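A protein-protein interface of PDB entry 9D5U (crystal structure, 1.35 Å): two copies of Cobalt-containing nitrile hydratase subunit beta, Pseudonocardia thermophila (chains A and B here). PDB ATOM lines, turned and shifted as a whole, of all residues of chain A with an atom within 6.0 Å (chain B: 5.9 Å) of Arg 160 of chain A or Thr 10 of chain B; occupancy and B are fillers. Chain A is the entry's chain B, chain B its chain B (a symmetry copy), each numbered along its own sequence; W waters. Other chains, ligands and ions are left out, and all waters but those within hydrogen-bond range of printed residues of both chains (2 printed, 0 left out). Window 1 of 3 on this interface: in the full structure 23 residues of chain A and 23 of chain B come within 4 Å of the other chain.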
ATOM      1  N   MET A   1     -17.304 -11.752 -23.020  1.00  0.00           N
ATOM      2  CA  MET A   1     -17.165 -10.601 -23.918  1.00  0.00           C
ATOM      3  C   MET A   1     -17.698  -9.325 -23.305  1.00  0.00           C
ATOM      4  O   MET A   1     -18.424  -9.339 -22.306  1.00  0.00           O
ATOM      5  CB  MET A   1     -17.972 -10.790 -25.216  1.00  0.00           C
ATOM      6  CG  MET A   1     -19.476 -11.153 -25.011  1.00  0.00           C
ATOM      7  SD  MET A   1     -20.665 -10.604 -26.284  1.00  0.00           S
ATOM      8  CE  MET A   1     -19.724 -10.780 -27.820  1.00  0.00           C
ATOM      9  N   ASN A   2     -17.381  -8.220 -23.973  1.00  0.00           N
ATOM     10  CA  ASN A   2     -17.900  -6.907 -23.625  1.00  0.00           C
ATOM     11  C   ASN A   2     -19.273  -6.668 -24.270  1.00  0.00           C
ATOM     12  O   ASN A   2     -19.507  -5.634 -24.904  1.00  0.00           O
ATOM     13  CB  ASN A   2     -16.915  -5.840 -24.080  1.00  0.00           C
ATOM     14  CG  ASN A   2     -15.588  -5.903 -23.343  1.00  0.00           C
ATOM     15  OD1 ASN A   2     -15.431  -6.682 -22.390  1.00  0.00           O
ATOM     16  ND2 ASN A   2     -14.625  -5.056 -23.762  1.00  0.00           N
ATOM     17  N   GLY A   3     -20.203  -7.639 -24.128  1.00  0.00           N
ATOM     18  CA  GLY A   3     -21.497  -7.509 -24.760  1.00  0.00           C
ATOM     19  C   GLY A   3     -22.481  -6.650 -23.983  1.00  0.00           C
ATOM     20  O   GLY A   3     -22.309  -6.348 -22.792  1.00  0.00           O
ATOM     21  N   VAL A   4     -23.556  -6.262 -24.685  1.00  0.00           N
ATOM     22  CA  VAL A   4     -24.570  -5.385 -24.092  1.00  0.00           C
ATOM     23  C   VAL A   4     -25.280  -6.064 -22.930  1.00  0.00           C
ATOM     24  O   VAL A   4     -25.784  -5.390 -22.022  1.00  0.00           O
ATOM     25  CB  VAL A   4     -25.562  -4.854 -25.157  1.00  0.00           C
ATOM     26  CG1 VAL A   4     -26.700  -4.097 -24.490  1.00  0.00           C
ATOM     27  CG2 VAL A   4     -24.853  -3.944 -26.158  1.00  0.00           C
ATOM     28  N   TYR A   5     -25.337  -7.396 -22.942  1.00  0.00           N
ATOM     29  CA  TYR A   5     -25.974  -8.150 -21.872  1.00  0.00           C
ATOM     30  C   TYR A   5     -25.382  -7.807 -20.497  1.00  0.00           C
ATOM     31  O   TYR A   5     -26.080  -7.893 -19.479  1.00  0.00           O
ATOM     32  CB  TYR A   5     -25.792  -9.634 -22.172  1.00  0.00           C
ATOM     33  CG  TYR A   5     -24.375 -10.095 -21.891  1.00  0.00           C
ATOM     34  CD1 TYR A   5     -23.382  -9.966 -22.852  1.00  0.00           C
ATOM     35  CD2 TYR A   5     -24.020 -10.605 -20.635  1.00  0.00           C
ATOM     36  CE1 TYR A   5     -22.075 -10.362 -22.583  1.00  0.00           C
ATOM     37  CE2 TYR A   5     -22.733 -10.999 -20.360  1.00  0.00           C
ATOM     38  CZ  TYR A   5     -21.755 -10.874 -21.326  1.00  0.00           C
ATOM     39  OH  TYR A   5     -20.463 -11.291 -21.034  1.00  0.00           O
ATOM     40  N   ASP A   6     -24.093  -7.448 -20.446  1.00  0.00           N
ATOM     41  CA  ASP A   6     -23.391  -7.073 -19.209  1.00  0.00           C
ATOM     42  C   ASP A   6     -23.847  -5.664 -18.819  1.00  0.00           C
ATOM     43  O   ASP A   6     -23.175  -4.649 -19.053  1.00  0.00           O
ATOM     44  CB  ASP A   6     -21.888  -7.192 -19.448  1.00  0.00           C
ATOM     45  CG  ASP A   6     -21.041  -6.629 -18.321  1.00  0.00           C
ATOM     46  OD1 ASP A   6     -21.527  -6.419 -17.179  1.00  0.00           O
ATOM     47  OD2 ASP A   6     -19.849  -6.353 -18.626  1.00  0.00           O
ATOM     48  N   VAL A   7     -25.046  -5.604 -18.217  1.00  0.00           N
ATOM     49  CA  VAL A   7     -25.788  -4.337 -18.059  1.00  0.00           C
ATOM     50  C   VAL A   7     -25.606  -3.665 -16.693  1.00  0.00           C
ATOM     51  O   VAL A   7     -26.100  -2.535 -16.502  1.00  0.00           O
ATOM     52  CB  VAL A   7     -27.297  -4.504 -18.368  1.00  0.00           C
ATOM     53  CG1 VAL A   7     -27.485  -5.062 -19.766  1.00  0.00           C
ATOM     54  CG2 VAL A   7     -27.962  -5.437 -17.318  1.00  0.00           C
ATOM     55  N   GLY A   8     -24.925  -4.318 -15.744  1.00  0.00           N
ATOM     56  CA  GLY A   8     -24.715  -3.714 -14.439  1.00  0.00           C
ATOM     57  C   GLY A   8     -24.086  -2.347 -14.538  1.00  0.00           C
ATOM     58  O   GLY A   8     -23.017  -2.188 -15.124  1.00  0.00           O
ATOM     59  N   THR A  10     -25.303   0.228 -16.207  1.00  0.00           N
ATOM     60  CA  THR A  10     -25.772   0.960 -17.377  1.00  0.00           C
ATOM     61  C   THR A  10     -26.925   1.909 -17.026  1.00  0.00           C
ATOM     62  O   THR A  10     -27.816   1.576 -16.237  1.00  0.00           O
ATOM     63  CB  THR A  10     -26.213  -0.034 -18.456  1.00  0.00           C
ATOM     64  OG1 THR A  10     -25.077  -0.756 -18.931  1.00  0.00           O
ATOM     65  CG2 THR A  10     -26.870   0.686 -19.634  1.00  0.00           C
ATOM     66  N   LYS A 153     -12.648 -11.924 -25.316  1.00  0.00           N
ATOM     67  CA  LYS A 153     -13.728 -11.861 -26.301  1.00  0.00           C
ATOM     68  C   LYS A 153     -14.738 -12.979 -26.078  1.00  0.00           C
ATOM     69  O   LYS A 153     -15.922 -12.814 -26.413  1.00  0.00           O
ATOM     70  CB  LYS A 153     -13.172 -11.960 -27.734  1.00  0.00           C
ATOM     71  CG  LYS A 153     -12.407 -10.736 -28.198  1.00  0.00           C
ATOM     72  CD  LYS A 153     -13.299  -9.563 -28.504  1.00  0.00           C
ATOM     73  CE  LYS A 153     -14.100  -9.778 -29.776  1.00  0.00           C
ATOM     74  NZ  LYS A 153     -15.366  -9.002 -29.702  1.00  0.00           N
ATOM     75  N   ARG A 158     -17.062 -11.594 -16.044  1.00  0.00           N
ATOM     76  CA  ARG A 158     -16.261 -10.434 -15.663  1.00  0.00           C
ATOM     77  C   ARG A 158     -17.058  -9.175 -15.973  1.00  0.00           C
ATOM     78  O   ARG A 158     -16.705  -8.410 -16.872  1.00  0.00           O
ATOM     79  CB  ARG A 158     -14.885 -10.437 -16.391  1.00  0.00           C
ATOM     80  CG  ARG A 158     -14.091 -11.700 -16.167  1.00  0.00           C
ATOM     81  CD  ARG A 158     -12.952 -11.859 -17.166  1.00  0.00           C
ATOM     82  NE  ARG A 158     -12.151 -13.051 -16.901  1.00  0.00           N
ATOM     83  CZ  ARG A 158     -10.976 -13.043 -16.282  1.00  0.00           C
ATOM     84  NH1 ARG A 158     -10.465 -11.924 -15.785  1.00  0.00           N
ATOM     85  NH2 ARG A 158     -10.307 -14.185 -16.150  1.00  0.00           N
ATOM     86  N   ALA A 159     -18.134  -8.952 -15.221  1.00  0.00           N
ATOM     87  CA  ALA A 159     -18.890  -7.723 -15.376  1.00  0.00           C
ATOM     88  C   ALA A 159     -17.941  -6.540 -15.467  1.00  0.00           C
ATOM     89  O   ALA A 159     -16.953  -6.460 -14.721  1.00  0.00           O
ATOM     90  CB  ALA A 159     -19.835  -7.549 -14.189  1.00  0.00           C
ATOM     91  N   ARG A 160     -18.242  -5.616 -16.395  1.00  0.00           N
ATOM     92  CA  ARG A 160     -17.337  -4.499 -16.653  1.00  0.00           C
ATOM     93  C   ARG A 160     -17.264  -3.507 -15.478  1.00  0.00           C
ATOM     94  O   ARG A 160     -16.251  -2.814 -15.305  1.00  0.00           O
ATOM     95  CB  ARG A 160     -17.779  -3.790 -17.921  1.00  0.00           C
ATOM     96  CG  ARG A 160     -17.162  -4.341 -19.186  1.00  0.00           C
ATOM     97  CD  ARG A 160     -17.867  -3.740 -20.401  1.00  0.00           C
ATOM     98  NE  ARG A 160     -19.324  -3.895 -20.364  1.00  0.00           N
ATOM     99  CZ  ARG A 160     -20.159  -3.291 -21.207  1.00  0.00           C
ATOM    100  NH1 ARG A 160     -19.722  -2.419 -22.114  1.00  0.00           N
ATOM    101  NH2 ARG A 160     -21.467  -3.570 -21.146  1.00  0.00           N
ATOM    102  N   TYR A 161     -18.320  -3.427 -14.659  1.00  0.00           N
ATOM    103  CA  TYR A 161     -18.345  -2.498 -13.540  1.00  0.00           C
ATOM    104  C   TYR A 161     -17.428  -2.910 -12.389  1.00  0.00           C
ATOM    105  O   TYR A 161     -17.155  -2.060 -11.528  1.00  0.00           O
ATOM    106  CB  TYR A 161     -19.804  -2.204 -13.084  1.00  0.00           C
ATOM    107  CG  TYR A 161     -20.448  -3.268 -12.194  1.00  0.00           C
ATOM    108  CD1 TYR A 161     -21.139  -4.353 -12.740  1.00  0.00           C
ATOM    109  CD2 TYR A 161     -20.353  -3.200 -10.816  1.00  0.00           C
ATOM    110  CE1 TYR A 161     -21.712  -5.344 -11.931  1.00  0.00           C
ATOM    111  CE2 TYR A 161     -20.933  -4.177  -9.999  1.00  0.00           C
ATOM    112  CZ  TYR A 161     -21.613  -5.245 -10.557  1.00  0.00           C
ATOM    113  OH  TYR A 161     -22.190  -6.204  -9.736  1.00  0.00           O
ATOM    114  N   VAL A 162     -16.932  -4.161 -12.362  1.00  0.00           N
ATOM    115  CA  VAL A 162     -16.045  -4.617 -11.284  1.00  0.00           C
ATOM    116  C   VAL A 162     -14.582  -4.715 -11.695  1.00  0.00           C
ATOM    117  O   VAL A 162     -13.721  -4.912 -10.821  1.00  0.00           O
ATOM    118  CB  VAL A 162     -16.505  -5.949 -10.652  1.00  0.00           C
ATOM    119  CG1 VAL A 162     -17.913  -5.817 -10.074  1.00  0.00           C
ATOM    120  CG2 VAL A 162     -16.418  -7.080 -11.645  1.00  0.00           C
ATOM    121  N   ARG A 163     -14.269  -4.611 -12.987  1.00  0.00           N
ATOM    122  CA  ARG A 163     -12.902  -4.846 -13.431  1.00  0.00           C
ATOM    123  C   ARG A 163     -11.959  -3.761 -12.930  1.00  0.00           C
ATOM    124  O   ARG A 163     -12.279  -2.565 -12.945  1.00  0.00           O
ATOM    125  CB  ARG A 163     -12.858  -4.886 -14.943  1.00  0.00           C
ATOM    126  CG  ARG A 163     -13.682  -5.998 -15.517  1.00  0.00           C
ATOM    127  CD  ARG A 163     -13.384  -6.098 -16.986  1.00  0.00           C
ATOM    128  NE  ARG A 163     -14.367  -6.901 -17.684  1.00  0.00           N
ATOM    129  CZ  ARG A 163     -14.506  -6.904 -18.999  1.00  0.00           C
ATOM    130  NH1 ARG A 163     -13.729  -6.152 -19.773  1.00  0.00           N
ATOM    131  NH2 ARG A 163     -15.452  -7.673 -19.548  1.00  0.00           N
ATOM    132  N   VAL B   4     -25.990   3.419 -23.358  1.00  0.00           N
ATOM    133  CA  VAL B   4     -25.509   2.465 -24.361  1.00  0.00           C
ATOM    134  C   VAL B   4     -24.695   3.159 -25.442  1.00  0.00           C
ATOM    135  O   VAL B   4     -23.827   2.538 -26.070  1.00  0.00           O
ATOM    136  CB  VAL B   4     -26.666   1.620 -24.950  1.00  0.00           C
ATOM    137  CG1 VAL B   4     -26.166   0.769 -26.107  1.00  0.00           C
ATOM    138  CG2 VAL B   4     -27.287   0.722 -23.880  1.00  0.00           C
ATOM    139  N   ASP B   6     -22.290   5.067 -25.164  1.00  0.00           N
ATOM    140  CA  ASP B   6     -20.874   5.002 -24.772  1.00  0.00           C
ATOM    141  C   ASP B   6     -20.357   3.601 -25.114  1.00  0.00           C
ATOM    142  O   ASP B   6     -20.235   2.702 -24.270  1.00  0.00           O
ATOM    143  CB  ASP B   6     -20.763   5.357 -23.291  1.00  0.00           C
ATOM    144  CG  ASP B   6     -19.384   5.118 -22.705  1.00  0.00           C
ATOM    145  OD1 ASP B   6     -18.373   4.985 -23.443  1.00  0.00           O
ATOM    146  OD2 ASP B   6     -19.339   5.023 -21.449  1.00  0.00           O
ATOM    147  N   VAL B   7     -20.060   3.410 -26.410  1.00  0.00           N
ATOM    148  CA  VAL B   7     -19.858   2.064 -26.983  1.00  0.00           C
ATOM    149  C   VAL B   7     -18.389   1.633 -27.080  1.00  0.00           C
ATOM    150  O   VAL B   7     -18.121   0.470 -27.445  1.00  0.00           O
ATOM    151  CB  VAL B   7     -20.544   1.910 -28.364  1.00  0.00           C
ATOM    152  CG1 VAL B   7     -22.024   2.225 -28.248  1.00  0.00           C
ATOM    153  CG2 VAL B   7     -19.871   2.845 -29.408  1.00  0.00           C
ATOM    154  N   GLY B   8     -17.439   2.524 -26.774  1.00  0.00           N
ATOM    155  CA  GLY B   8     -16.034   2.156 -26.836  1.00  0.00           C
ATOM    156  C   GLY B   8     -15.731   0.925 -26.020  1.00  0.00           C
ATOM    157  O   GLY B   8     -16.004   0.883 -24.822  1.00  0.00           O
ATOM    158  N   GLY B   9     -15.181  -0.095 -26.659  1.00  0.00           N
ATOM    159  CA  GLY B   9     -14.838  -1.326 -25.971  1.00  0.00           C
ATOM    160  C   GLY B   9     -15.942  -2.353 -25.882  1.00  0.00           C
ATOM    161  O   GLY B   9     -15.691  -3.450 -25.363  1.00  0.00           O
ATOM    162  N   THR B  10     -17.148  -2.035 -26.378  1.00  0.00           N
ATOM    163  CA  THR B  10     -18.244  -2.995 -26.412  1.00  0.00           C
ATOM    164  C   THR B  10     -18.015  -4.079 -27.474  1.00  0.00           C
ATOM    165  O   THR B  10     -17.536  -3.806 -28.579  1.00  0.00           O
ATOM    166  CB  THR B  10     -19.559  -2.257 -26.683  1.00  0.00           C
ATOM    167  OG1 THR B  10     -19.870  -1.415 -25.574  1.00  0.00           O
ATOM    168  CG2 THR B  10     -20.709  -3.241 -26.897  1.00  0.00           C
ATOM    169  N   ASP B  11     -18.349  -5.310 -27.141  1.00  0.00           N
ATOM    170  CA  ASP B  11     -18.272  -6.394 -28.093  1.00  0.00           C
ATOM    171  C   ASP B  11     -19.653  -6.713 -28.677  1.00  0.00           C
ATOM    172  O   ASP B  11     -20.694  -6.277 -28.178  1.00  0.00           O
ATOM    173  CB  ASP B  11     -17.669  -7.651 -27.451  1.00  0.00           C
ATOM    174  CG  ASP B  11     -16.226  -7.484 -27.096  1.00  0.00           C
ATOM    175  OD1 ASP B  11     -15.530  -6.745 -27.826  1.00  0.00           O
ATOM    176  OD2 ASP B  11     -15.779  -8.117 -26.122  1.00  0.00           O
ATOM    177  N   GLY B  12     -19.639  -7.499 -29.754  1.00  0.00           N
ATOM    178  CA  GLY B  12     -20.845  -8.138 -30.249  1.00  0.00           C
ATOM    179  C   GLY B  12     -21.807  -7.231 -30.969  1.00  0.00           C
ATOM    180  O   GLY B  12     -22.984  -7.596 -31.100  1.00  0.00           O
ATOM    181  N   LEU B  13     -21.348  -6.054 -31.428  1.00  0.00           N
ATOM    182  CA  LEU B  13     -22.198  -5.131 -32.180  1.00  0.00           C
ATOM    183  C   LEU B  13     -22.309  -5.477 -33.673  1.00  0.00           C
ATOM    184  O   LEU B  13     -23.213  -4.961 -34.355  1.00  0.00           O
ATOM    185  CB  LEU B  13     -21.756  -3.675 -31.979  1.00  0.00           C
ATOM    186  CG  LEU B  13     -21.707  -3.232 -30.512  1.00  0.00           C
ATOM    187  CD1 LEU B  13     -21.640  -1.706 -30.338  1.00  0.00           C
ATOM    188  CD2 LEU B  13     -22.894  -3.807 -29.739  1.00  0.00           C
ATOM    189  N   ARG B 160     -16.692   4.907 -20.408  1.00  0.00           N
ATOM    190  CA  ARG B 160     -16.519   3.947 -19.320  1.00  0.00           C
ATOM    191  C   ARG B 160     -15.201   3.158 -19.426  1.00  0.00           C
ATOM    192  O   ARG B 160     -14.667   2.691 -18.408  1.00  0.00           O
ATOM    193  CB  ARG B 160     -17.706   3.001 -19.305  1.00  0.00           C
ATOM    194  CG  ARG B 160     -18.864   3.473 -18.456  1.00  0.00           C
ATOM    195  CD  ARG B 160     -20.083   2.591 -18.722  1.00  0.00           C
ATOM    196  NE  ARG B 160     -20.425   2.483 -20.143  1.00  0.00           N
ATOM    197  CZ  ARG B 160     -21.321   1.626 -20.631  1.00  0.00           C
ATOM    198  NH1 ARG B 160     -21.923   0.731 -19.851  1.00  0.00           N
ATOM    199  NH2 ARG B 160     -21.626   1.669 -21.934  1.00  0.00           N
HETATM  200  O   HOH W   1     -23.115  -1.179 -22.746  1.00  0.00           O
HETATM  201  O   HOH W   2     -23.377  -6.686 -27.503  1.00  0.00           O
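The backbone carbonyl oxygen (O) of Gly 9 of chain B lies within hydrogen-bond range of the side-chain amide nitrogen (ND2) of Asn 2 of chain A (2.5 Å). The backbone NH (N) of Asp 11 of chain B sits at hydrogen-bond distance from the backbone carbonyl oxygen (O) of Asn 2 of chain A. The side-chain amino group of Lys 153 of chain A lies within salt-bridge range of the side-chain carboxylate of Asp 11 of chain B.
Of chain B, only Thr 10 (3.6 Å) comes within 4 Å of Arg 160 of chain A. Of the printed residues of chain B, Thr 10 of chain A touches Arg 160 (3.6 Å). Of the printed residues of chain A, Gly 12 of chain B touches Met 1. Of the printed residues of chain A, Arg 160 of chain B touches Thr 10. Of the printed residues of chain A, Gly 9 of chain B touches Asn 2 (2.5 Å). Printed residues of chain B within 4 Å of Asn 2 of chain A: Gly 9, Thr 10 and Asp 11. The nearest residue of chain B that does not touch Arg 160 of chain A is Arg 160 of chain B (4.5 Å). The nearest printed residue of chain B that does not touch Met 1 of chain A is Leu 13 of chain B (6.2 Å).
SD of Met 1 of chain A sits close to N of Gly 3 of chain A (3.7 Å). OH of Tyr 5 of chain A lies within hydrogen-bond range of O of Met 1 of chain A (3.1 Å). NH2 of Arg 163 of chain A is in hydrogen-bond range of OD1 of Asn 2 of chain A, at 3.0 Å. O of Gly 3 of chain A lies within hydrogen-bond range of NH2 of Arg 160 of chain A, 3.3 Å away. The side-chain carboxylate (OD2) of Asp 6 of chain B lies within salt-bridge range of the guanidinium group (NE) of Arg 160 of chain B. The backbone carbonyl oxygen (O) of Val 7 of chain B sits close to the side-chain hydroxyl (OG1) of Thr 10 of chain B (3.2 Å).
Water W2 bridges O of Asp 11 of chain B (2.8 Å) and N of Val 4 of chain A (2.9 Å). Water W1 bridges NH2 of Arg 160 of chain A and NH2 of Arg 160 of chain B.
Thr 10 of chain A touches Arg 160 of chain B, and with the chains exchanged Arg 160 of chain A touches Thr 10 of chain B.
Hydrophobic or aromatic side chains of chain A that line the printed part of chain B: Met 1. Printed residues of chain B that touch a printed residue of chain A: Gly 9, Thr 10, Asp 11, Gly 12 and Arg 160. Along chain B the printed residues that touch a printed residue of chain A span positions 9 to 160.
CB of Met 1 of chain A touches OD2 of Asp 11 of chain B, 3.6 Å away. Met 1 of chain A touches Gly 12 of chain B. Asn 2 of chain A touches Thr 10 of chain B. CA of Gly 3 of chain A touches O of Asp 11 of chain B, 3.7 Å away. Thr 10 of chain A touches Arg 160 of chain B (OG1 to NH1, 3.6 Å). NH1 of Arg 160 of chain A touches OG1 of Thr 10 of chain B, 3.6 Å away.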
